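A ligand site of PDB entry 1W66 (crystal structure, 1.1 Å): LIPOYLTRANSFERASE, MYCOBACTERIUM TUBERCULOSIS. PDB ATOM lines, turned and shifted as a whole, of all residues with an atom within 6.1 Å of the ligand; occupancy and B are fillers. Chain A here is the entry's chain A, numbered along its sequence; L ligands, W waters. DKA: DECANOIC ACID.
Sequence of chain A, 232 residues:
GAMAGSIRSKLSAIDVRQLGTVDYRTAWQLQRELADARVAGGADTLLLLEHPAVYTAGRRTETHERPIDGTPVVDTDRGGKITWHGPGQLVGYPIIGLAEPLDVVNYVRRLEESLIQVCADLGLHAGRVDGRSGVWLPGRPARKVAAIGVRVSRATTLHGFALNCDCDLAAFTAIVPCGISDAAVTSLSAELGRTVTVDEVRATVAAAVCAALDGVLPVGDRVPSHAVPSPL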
ATOM      1  N   THR A  56     -15.240 -20.771  22.507  1.00  0.00           N
ATOM      2  CA  THR A  56     -14.272 -21.819  22.864  1.00  0.00           C
ATOM      3  C   THR A  56     -14.318 -22.892  21.786  1.00  0.00           C
ATOM      4  O   THR A  56     -15.365 -23.175  21.186  1.00  0.00           O
ATOM      5  CB  THR A  56     -14.483 -22.424  24.249  1.00  0.00           C
ATOM      6  OG1 THR A  56     -15.650 -23.250  24.193  1.00  0.00           O
ATOM      7  CG2 THR A  56     -14.651 -21.369  25.309  1.00  0.00           C
ATOM      8  N   ARG A  60     -11.218 -30.654  17.745  1.00  0.00           N
ATOM      9  CA  ARG A  60     -11.792 -31.009  16.462  1.00  0.00           C
ATOM     10  C   ARG A  60     -12.289 -29.803  15.624  1.00  0.00           C
ATOM     11  O   ARG A  60     -12.627 -29.973  14.475  1.00  0.00           O
ATOM     12  CB  ARG A  60     -12.948 -31.997  16.641  1.00  0.00           C
ATOM     13  CG  ARG A  60     -12.443 -33.353  17.098  1.00  0.00           C
ATOM     14  CD  ARG A  60     -13.640 -34.268  17.529  1.00  0.00           C
ATOM     15  NE  ARG A  60     -14.515 -34.365  16.373  1.00  0.00           N
ATOM     16  CZ  ARG A  60     -15.755 -33.888  16.268  1.00  0.00           C
ATOM     17  NH1 ARG A  60     -16.363 -34.031  15.100  1.00  0.00           N
ATOM     18  NH2 ARG A  60     -16.449 -33.370  17.266  1.00  0.00           N
ATOM     19  N   ARG A  78     -12.209 -29.931  26.136  1.00  0.00           N
ATOM     20  CA  ARG A  78     -13.461 -30.666  26.117  1.00  0.00           C
ATOM     21  C   ARG A  78     -13.690 -31.267  24.731  1.00  0.00           C
ATOM     22  O   ARG A  78     -13.147 -30.801  23.705  1.00  0.00           O
ATOM     23  CB  ARG A  78     -14.665 -29.757  26.469  1.00  0.00           C
ATOM     24  CG  ARG A  78     -14.695 -28.555  25.559  1.00  0.00           C
ATOM     25  CD  ARG A  78     -16.127 -28.053  25.413  1.00  0.00           C
ATOM     26  NE  ARG A  78     -16.172 -26.847  24.607  1.00  0.00           N
ATOM     27  CZ  ARG A  78     -16.070 -26.798  23.277  1.00  0.00           C
ATOM     28  NH1 ARG A  78     -16.019 -27.911  22.557  1.00  0.00           N
ATOM     29  NH2 ARG A  78     -16.071 -25.630  22.676  1.00  0.00           N
ATOM     30  N   GLY A  79     -14.560 -32.308  24.692  1.00  0.00           N
ATOM     31  CA  GLY A  79     -15.061 -32.748  23.425  1.00  0.00           C
ATOM     32  C   GLY A  79     -15.843 -31.654  22.717  1.00  0.00           C
ATOM     33  O   GLY A  79     -16.403 -30.727  23.245  1.00  0.00           O
ATOM     34  N   GLY A  80     -16.022 -31.894  21.429  1.00  0.00           N
ATOM     35  CA  GLY A  80     -16.803 -31.033  20.571  1.00  0.00           C
ATOM     36  C   GLY A  80     -15.970 -29.994  19.826  1.00  0.00           C
ATOM     37  O   GLY A  80     -14.776 -29.867  20.012  1.00  0.00           O
ATOM     38  N   LYS A  81     -16.617 -29.233  18.983  1.00  0.00           N
ATOM     39  CA  LYS A  81     -16.043 -28.221  18.115  1.00  0.00           C
ATOM     40  C   LYS A  81     -16.189 -26.851  18.778  1.00  0.00           C
ATOM     41  O   LYS A  81     -15.786 -26.706  19.937  1.00  0.00           O
ATOM     42  CB  LYS A  81     -16.570 -28.385  16.721  1.00  0.00           C
ATOM     43  CG  LYS A  81     -16.154 -29.658  16.020  1.00  0.00           C
ATOM     44  CD  LYS A  81     -16.753 -29.809  14.638  1.00  0.00           C
ATOM     45  CE  LYS A  81     -15.769 -30.463  13.651  1.00  0.00           C
ATOM     46  NZ  LYS A  81     -16.355 -30.393  12.296  1.00  0.00           N
ATOM     47  N   ILE A  82     -16.742 -25.860  18.102  1.00  0.00           N
ATOM     48  CA  ILE A  82     -16.789 -24.503  18.608  1.00  0.00           C
ATOM     49  C   ILE A  82     -18.154 -24.194  19.194  1.00  0.00           C
ATOM     50  O   ILE A  82     -19.204 -24.623  18.680  1.00  0.00           O
ATOM     51  CB  ILE A  82     -16.375 -23.495  17.552  1.00  0.00           C
ATOM     52  CG1 ILE A  82     -16.140 -22.117  18.117  1.00  0.00           C
ATOM     53  CG2 ILE A  82     -17.376 -23.365  16.444  1.00  0.00           C
ATOM     54  CD1 ILE A  82     -15.371 -21.195  17.205  1.00  0.00           C
ATOM     55  N   THR A  83     -18.164 -23.407  20.249  1.00  0.00           N
ATOM     56  CA  THR A  83     -19.386 -22.894  20.841  1.00  0.00           C
ATOM     57  C   THR A  83     -19.120 -21.503  21.422  1.00  0.00           C
ATOM     58  O   THR A  83     -17.999 -20.988  21.372  1.00  0.00           O
ATOM     59  CB  THR A  83     -19.944 -23.865  21.911  1.00  0.00           C
ATOM     60  OG1 THR A  83     -21.352 -23.538  22.079  1.00  0.00           O
ATOM     61  CG2 THR A  83     -19.246 -23.763  23.246  1.00  0.00           C
ATOM     62  N   HIS A  85     -20.187 -19.031  24.933  1.00  0.00           N
ATOM     63  CA  HIS A  85     -20.760 -18.841  26.253  1.00  0.00           C
ATOM     64  C   HIS A  85     -20.866 -17.346  26.520  1.00  0.00           C
ATOM     65  O   HIS A  85     -20.038 -16.592  26.028  1.00  0.00           O
ATOM     66  CB  HIS A  85     -19.930 -19.489  27.376  1.00  0.00           C
ATOM     67  CG  HIS A  85     -19.587 -20.922  27.105  1.00  0.00           C
ATOM     68  ND1 HIS A  85     -20.537 -21.895  26.979  1.00  0.00           N
ATOM     69  CD2 HIS A  85     -18.398 -21.562  26.959  1.00  0.00           C
ATOM     70  CE1 HIS A  85     -19.916 -23.046  26.778  1.00  0.00           C
ATOM     71  NE2 HIS A  85     -18.622 -22.908  26.758  1.00  0.00           N
ATOM     72  N   VAL A  91     -24.031 -22.314  32.551  1.00  0.00           N
ATOM     73  CA  VAL A  91     -22.978 -23.311  32.289  1.00  0.00           C
ATOM     74  C   VAL A  91     -22.883 -24.192  33.505  1.00  0.00           C
ATOM     75  O   VAL A  91     -22.789 -23.701  34.655  1.00  0.00           O
ATOM     76  CB  VAL A  91     -21.662 -22.603  31.974  1.00  0.00           C
ATOM     77  CG1 VAL A  91     -20.536 -23.589  31.793  1.00  0.00           C
ATOM     78  CG2 VAL A  91     -21.807 -21.795  30.711  1.00  0.00           C
ATOM     79  N   GLY A  92     -22.897 -25.499  33.304  1.00  0.00           N
ATOM     80  CA  GLY A  92     -22.720 -26.463  34.333  1.00  0.00           C
ATOM     81  C   GLY A  92     -21.501 -27.317  34.112  1.00  0.00           C
ATOM     82  O   GLY A  92     -21.316 -27.876  33.019  1.00  0.00           O
ATOM     83  N   TYR A  93     -20.685 -27.459  35.136  1.00  0.00           N
ATOM     84  CA  TYR A  93     -19.511 -28.278  35.116  1.00  0.00           C
ATOM     85  C   TYR A  93     -19.619 -29.322  36.226  1.00  0.00           C
ATOM     86  O   TYR A  93     -19.267 -29.080  37.376  1.00  0.00           O
ATOM     87  CB  TYR A  93     -18.264 -27.442  35.302  1.00  0.00           C
ATOM     88  CG  TYR A  93     -17.966 -26.452  34.202  1.00  0.00           C
ATOM     89  CD1 TYR A  93     -18.069 -26.823  32.867  1.00  0.00           C
ATOM     90  CD2 TYR A  93     -17.554 -25.182  34.462  1.00  0.00           C
ATOM     91  CE1 TYR A  93     -17.781 -25.938  31.835  1.00  0.00           C
ATOM     92  CE2 TYR A  93     -17.216 -24.283  33.433  1.00  0.00           C
ATOM     93  CZ  TYR A  93     -17.323 -24.666  32.129  1.00  0.00           C
ATOM     94  OH  TYR A  93     -16.979 -23.875  31.074  1.00  0.00           O
ATOM     95  N   GLY A 131     -26.601 -38.449  17.386  1.00  0.00           N
ATOM     96  CA  GLY A 131     -25.347 -38.070  16.713  1.00  0.00           C
ATOM     97  C   GLY A 131     -25.027 -36.583  16.905  1.00  0.00           C
ATOM     98  O   GLY A 131     -23.939 -36.153  16.512  1.00  0.00           O
ATOM     99  N   ARG A 132     -25.945 -35.800  17.461  1.00  0.00           N
ATOM    100  CA  ARG A 132     -25.738 -34.355  17.678  1.00  0.00           C
ATOM    101  C   ARG A 132     -26.033 -34.088  19.141  1.00  0.00           C
ATOM    102  O   ARG A 132     -27.148 -33.745  19.518  1.00  0.00           O
ATOM    103  CB  ARG A 132     -26.636 -33.562  16.744  1.00  0.00           C
ATOM    104  CG  ARG A 132     -26.326 -33.759  15.291  1.00  0.00           C
ATOM    105  CD  ARG A 132     -27.234 -32.878  14.412  1.00  0.00           C
ATOM    106  NE  ARG A 132     -26.855 -32.971  13.014  1.00  0.00           N
ATOM    107  CZ  ARG A 132     -27.227 -32.189  12.049  1.00  0.00           C
ATOM    108  NH1 ARG A 132     -28.078 -31.194  12.309  1.00  0.00           N
ATOM    109  NH2 ARG A 132     -26.806 -32.357  10.813  1.00  0.00           N
ATOM    110  N   SER A 133     -25.054 -34.267  20.007  1.00  0.00           N
ATOM    111  CA  SER A 133     -25.278 -34.213  21.461  1.00  0.00           C
ATOM    112  C   SER A 133     -25.865 -32.870  21.877  1.00  0.00           C
ATOM    113  O   SER A 133     -25.576 -31.877  21.264  1.00  0.00           O
ATOM    114  CB  SER A 133     -24.026 -34.427  22.293  1.00  0.00           C
ATOM    115  OG  SER A 133     -23.110 -33.379  22.103  1.00  0.00           O
ATOM    116  N   LYS A 144     -31.391 -25.953  18.784  1.00  0.00           N
ATOM    117  CA  LYS A 144     -30.605 -26.455  19.909  1.00  0.00           C
ATOM    118  C   LYS A 144     -30.654 -25.496  21.089  1.00  0.00           C
ATOM    119  O   LYS A 144     -30.232 -24.324  20.938  1.00  0.00           O
ATOM    120  CB  LYS A 144     -29.160 -26.673  19.446  1.00  0.00           C
ATOM    121  CG  LYS A 144     -28.347 -27.411  20.528  1.00  0.00           C
ATOM    122  CD  LYS A 144     -26.931 -27.726  19.944  1.00  0.00           C
ATOM    123  CE  LYS A 144     -26.098 -28.436  20.902  1.00  0.00           C
ATOM    124  NZ  LYS A 144     -24.723 -28.598  20.210  1.00  0.00           N
ATOM    125  N   ALA A 147     -26.067 -27.234  24.823  1.00  0.00           N
ATOM    126  CA  ALA A 147     -24.902 -27.905  24.294  1.00  0.00           C
ATOM    127  C   ALA A 147     -24.190 -28.663  25.370  1.00  0.00           C
ATOM    128  O   ALA A 147     -24.222 -28.296  26.553  1.00  0.00           O
ATOM    129  CB  ALA A 147     -23.963 -26.875  23.704  1.00  0.00           C
ATOM    130  N   ILE A 148     -23.520 -29.726  24.942  1.00  0.00           N
ATOM    131  CA  ILE A 148     -22.744 -30.589  25.832  1.00  0.00           C
ATOM    132  C   ILE A 148     -21.353 -30.784  25.226  1.00  0.00           C
ATOM    133  O   ILE A 148     -21.202 -31.038  24.029  1.00  0.00           O
ATOM    134  CB  ILE A 148     -23.393 -31.935  26.050  1.00  0.00           C
ATOM    135  CG1 ILE A 148     -24.781 -31.673  26.719  1.00  0.00           C
ATOM    136  CG2 ILE A 148     -22.526 -32.828  26.915  1.00  0.00           C
ATOM    137  CD1 ILE A 148     -25.715 -32.758  26.829  1.00  0.00           C
ATOM    138  N   GLY A 149     -20.350 -30.699  26.078  1.00  0.00           N
ATOM    139  CA  GLY A 149     -18.967 -30.996  25.692  1.00  0.00           C
ATOM    140  C   GLY A 149     -18.228 -31.348  26.942  1.00  0.00           C
ATOM    141  O   GLY A 149     -18.077 -30.507  27.823  1.00  0.00           O
ATOM    142  N   VAL A 150     -17.769 -32.579  27.036  1.00  0.00           N
ATOM    143  CA  VAL A 150     -17.181 -33.113  28.241  1.00  0.00           C
ATOM    144  C   VAL A 150     -15.834 -33.769  27.918  1.00  0.00           C
ATOM    145  O   VAL A 150     -15.461 -34.018  26.788  1.00  0.00           O
ATOM    146  CB  VAL A 150     -18.102 -34.158  28.939  1.00  0.00           C
ATOM    147  CG1 VAL A 150     -19.449 -33.530  29.240  1.00  0.00           C
ATOM    148  CG2 VAL A 150     -18.211 -35.422  28.136  1.00  0.00           C
ATOM    149  N   HIS A 159     -15.543 -30.353  32.239  1.00  0.00           N
ATOM    150  CA  HIS A 159     -16.418 -29.610  31.350  1.00  0.00           C
ATOM    151  C   HIS A 159     -17.845 -29.994  31.614  1.00  0.00           C
ATOM    152  O   HIS A 159     -18.194 -30.228  32.793  1.00  0.00           O
ATOM    153  CB  HIS A 159     -15.900 -29.628  29.913  1.00  0.00           C
ATOM    154  CG  HIS A 159     -14.559 -29.012  29.843  1.00  0.00           C
ATOM    155  ND1 HIS A 159     -14.333 -27.649  29.933  1.00  0.00           N
ATOM    156  CD2 HIS A 159     -13.350 -29.620  29.715  1.00  0.00           C
ATOM    157  CE1 HIS A 159     -13.019 -27.435  29.821  1.00  0.00           C
ATOM    158  NE2 HIS A 159     -12.402 -28.620  29.710  1.00  0.00           N
ATOM    159  N   GLY A 160     -18.755 -29.963  30.641  1.00  0.00           N
ATOM    160  CA  GLY A 160     -20.150 -30.107  31.001  1.00  0.00           C
ATOM    161  C   GLY A 160     -21.111 -29.656  29.961  1.00  0.00           C
ATOM    162  O   GLY A 160     -21.100 -30.158  28.826  1.00  0.00           O
ATOM    163  N   PHE A 161     -22.006 -28.761  30.336  1.00  0.00           N
ATOM    164  CA  PHE A 161     -23.105 -28.372  29.487  1.00  0.00           C
ATOM    165  C   PHE A 161     -23.323 -26.847  29.571  1.00  0.00           C
ATOM    166  O   PHE A 161     -22.872 -26.183  30.510  1.00  0.00           O
ATOM    167  CB  PHE A 161     -24.385 -29.131  29.876  1.00  0.00           C
ATOM    168  CG  PHE A 161     -24.851 -28.875  31.274  1.00  0.00           C
ATOM    169  CD1 PHE A 161     -25.614 -27.744  31.597  1.00  0.00           C
ATOM    170  CD2 PHE A 161     -24.572 -29.768  32.290  1.00  0.00           C
ATOM    171  CE1 PHE A 161     -26.040 -27.539  32.896  1.00  0.00           C
ATOM    172  CE2 PHE A 161     -25.011 -29.554  33.570  1.00  0.00           C
ATOM    173  CZ  PHE A 161     -25.764 -28.451  33.871  1.00  0.00           C
ATOM    174  N   ALA A 162     -24.128 -26.358  28.650  1.00  0.00           N
ATOM    175  CA  ALA A 162     -24.512 -24.963  28.622  1.00  0.00           C
ATOM    176  C   ALA A 162     -25.932 -24.865  28.155  1.00  0.00           C
ATOM    177  O   ALA A 162     -26.264 -25.319  27.064  1.00  0.00           O
ATOM    178  CB  ALA A 162     -23.580 -24.167  27.701  1.00  0.00           C
ATOM    179  N   PRO A 177     -21.789 -23.692  14.769  1.00  0.00           N
ATOM    180  CA  PRO A 177     -21.777 -24.197  16.155  1.00  0.00           C
ATOM    181  C   PRO A 177     -21.762 -25.697  16.225  1.00  0.00           C
ATOM    182  O   PRO A 177     -22.616 -26.376  15.641  1.00  0.00           O
ATOM    183  CB  PRO A 177     -23.064 -23.630  16.749  1.00  0.00           C
ATOM    184  CG  PRO A 177     -23.865 -23.248  15.581  1.00  0.00           C
ATOM    185  CD  PRO A 177     -23.053 -23.091  14.389  1.00  0.00           C
ATOM    186  N   CYS A 178     -20.772 -26.258  16.912  1.00  0.00           N
ATOM    187  CA  CYS A 178     -20.639 -27.692  17.068  1.00  0.00           C
ATOM    188  C   CYS A 178     -20.674 -28.429  15.738  1.00  0.00           C
ATOM    189  O   CYS A 178     -21.160 -29.533  15.638  1.00  0.00           O
ATOM    190  CB  CYS A 178     -21.696 -28.219  18.009  1.00  0.00           C
ATOM    191  SG  CYS A 178     -21.509 -27.587  19.676  1.00  0.00           S
ATOM    192  N   GLY A 179     -20.101 -27.832  14.732  1.00  0.00           N
ATOM    193  CA  GLY A 179     -19.959 -28.393  13.413  1.00  0.00           C
ATOM    194  C   GLY A 179     -21.264 -28.489  12.637  1.00  0.00           C
ATOM    195  O   GLY A 179     -21.255 -29.104  11.548  1.00  0.00           O
HETATM  196  C1  DKA L   1     -19.954 -30.798  19.149  1.00  0.00           C
HETATM  197  O1  DKA L   1     -19.106 -30.456  18.314  1.00  0.00           O
HETATM  198  C2  DKA L   1     -20.325 -29.940  20.353  1.00  0.00           C
HETATM  199  C3  DKA L   1     -19.995 -28.484  20.178  1.00  0.00           C
HETATM  200  C4  DKA L   1     -19.396 -27.871  21.396  1.00  0.00           C
HETATM  201  C5  DKA L   1     -20.328 -27.694  22.548  1.00  0.00           C
HETATM  202  C6  DKA L   1     -19.554 -27.444  23.877  1.00  0.00           C
HETATM  203  C7  DKA L   1     -20.432 -27.143  25.066  1.00  0.00           C
HETATM  204  C8  DKA L   1     -19.635 -26.957  26.308  1.00  0.00           C
HETATM  205  C9  DKA L   1     -20.447 -26.776  27.584  1.00  0.00           C
HETATM  206  C10 DKA L   1     -19.664 -26.518  28.780  1.00  0.00           C
HETATM  207  O2  DKA L   1     -20.593 -31.870  19.134  1.00  0.00           O
HETATM  208  O   HOH W   1     -20.658 -33.571  21.527  1.00  0.00           O
HETATM  209  O   HOH W   2     -20.154 -34.330  18.494  1.00  0.00           O
HETATM  210  O   HOH W   3     -22.844 -31.937  17.350  1.00  0.00           O
HETATM  211  O   HOH W   4     -18.778 -32.256  16.208  1.00  0.00           O
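N of Lys 81 lies within hydrogen-bond range of O1 of the ligand, at 2.9 Å. SG of Cys 178 is covalently linked to C3 of the ligand (1.8 Å).
N of Gly 149 is in hydrogen-bond range of O of Gly 160, at 2.9 Å. O of Phe 161 lies within hydrogen-bond range of N of Gly 92 (2.9 Å). O of Gly 80 lies close to NH1 of Arg 78 (3.4 Å). The backbone carbonyl oxygen (O) of Ala 147 is in hydrogen-bond range of the backbone NH (N) of Ala 162 (2.9 Å). The side-chain sulfur of Cys 178 lies within hydrogen-bond range of the side-chain amino group of Lys 144 (3.4 Å). The guanidinium group (NH2) of Arg 78 sits at hydrogen-bond distance from the side-chain hydroxyl (OG1) of Thr 56 (2.9 Å). O of Ile 82 lies within hydrogen-bond range of N of Cys 178 (2.9 Å). The backbone carbonyl oxygen of Lys 81 sits at hydrogen-bond distance from the guanidinium group of Arg 78.
Residues that only touch the ligand: Gly 80 (3.3 Å), Phe 161 (3.5 Å), Arg 78 (3.5 Å), Tyr 93 (3.6 Å), Gly 160 (3.7 Å), Gly 149 (3.7 Å), Thr 83 (3.7 Å), Ile 148 (3.8 Å), Ala 147 (3.8 Å), His 85 (3.9 Å) and Ala 162 (3.9 Å). Hydrophobic or aromatic side chains that line the ligand: His 85, Tyr 93 and Ala 147. Within 4 Å of the ligand: Arg 78, Gly 80, Lys 81, Thr 83, His 85, Tyr 93, Ala 147, Ile 148, Gly 149, Gly 160, Phe 161, Ala 162 and Cys 178.
Water W4 lies within hydrogen-bond range of an oxygen (O1) of the ligand (2.8 Å) and the guanidinium group (NH2) of Arg 60 (2.8 Å). Water W3 bridges O2 of the ligand (2.9 Å) and O of Cys 178 (3.4 Å). Water W1 bridges OG of Ser 133 (2.5 Å) and O2 of the ligand (2.9 Å).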
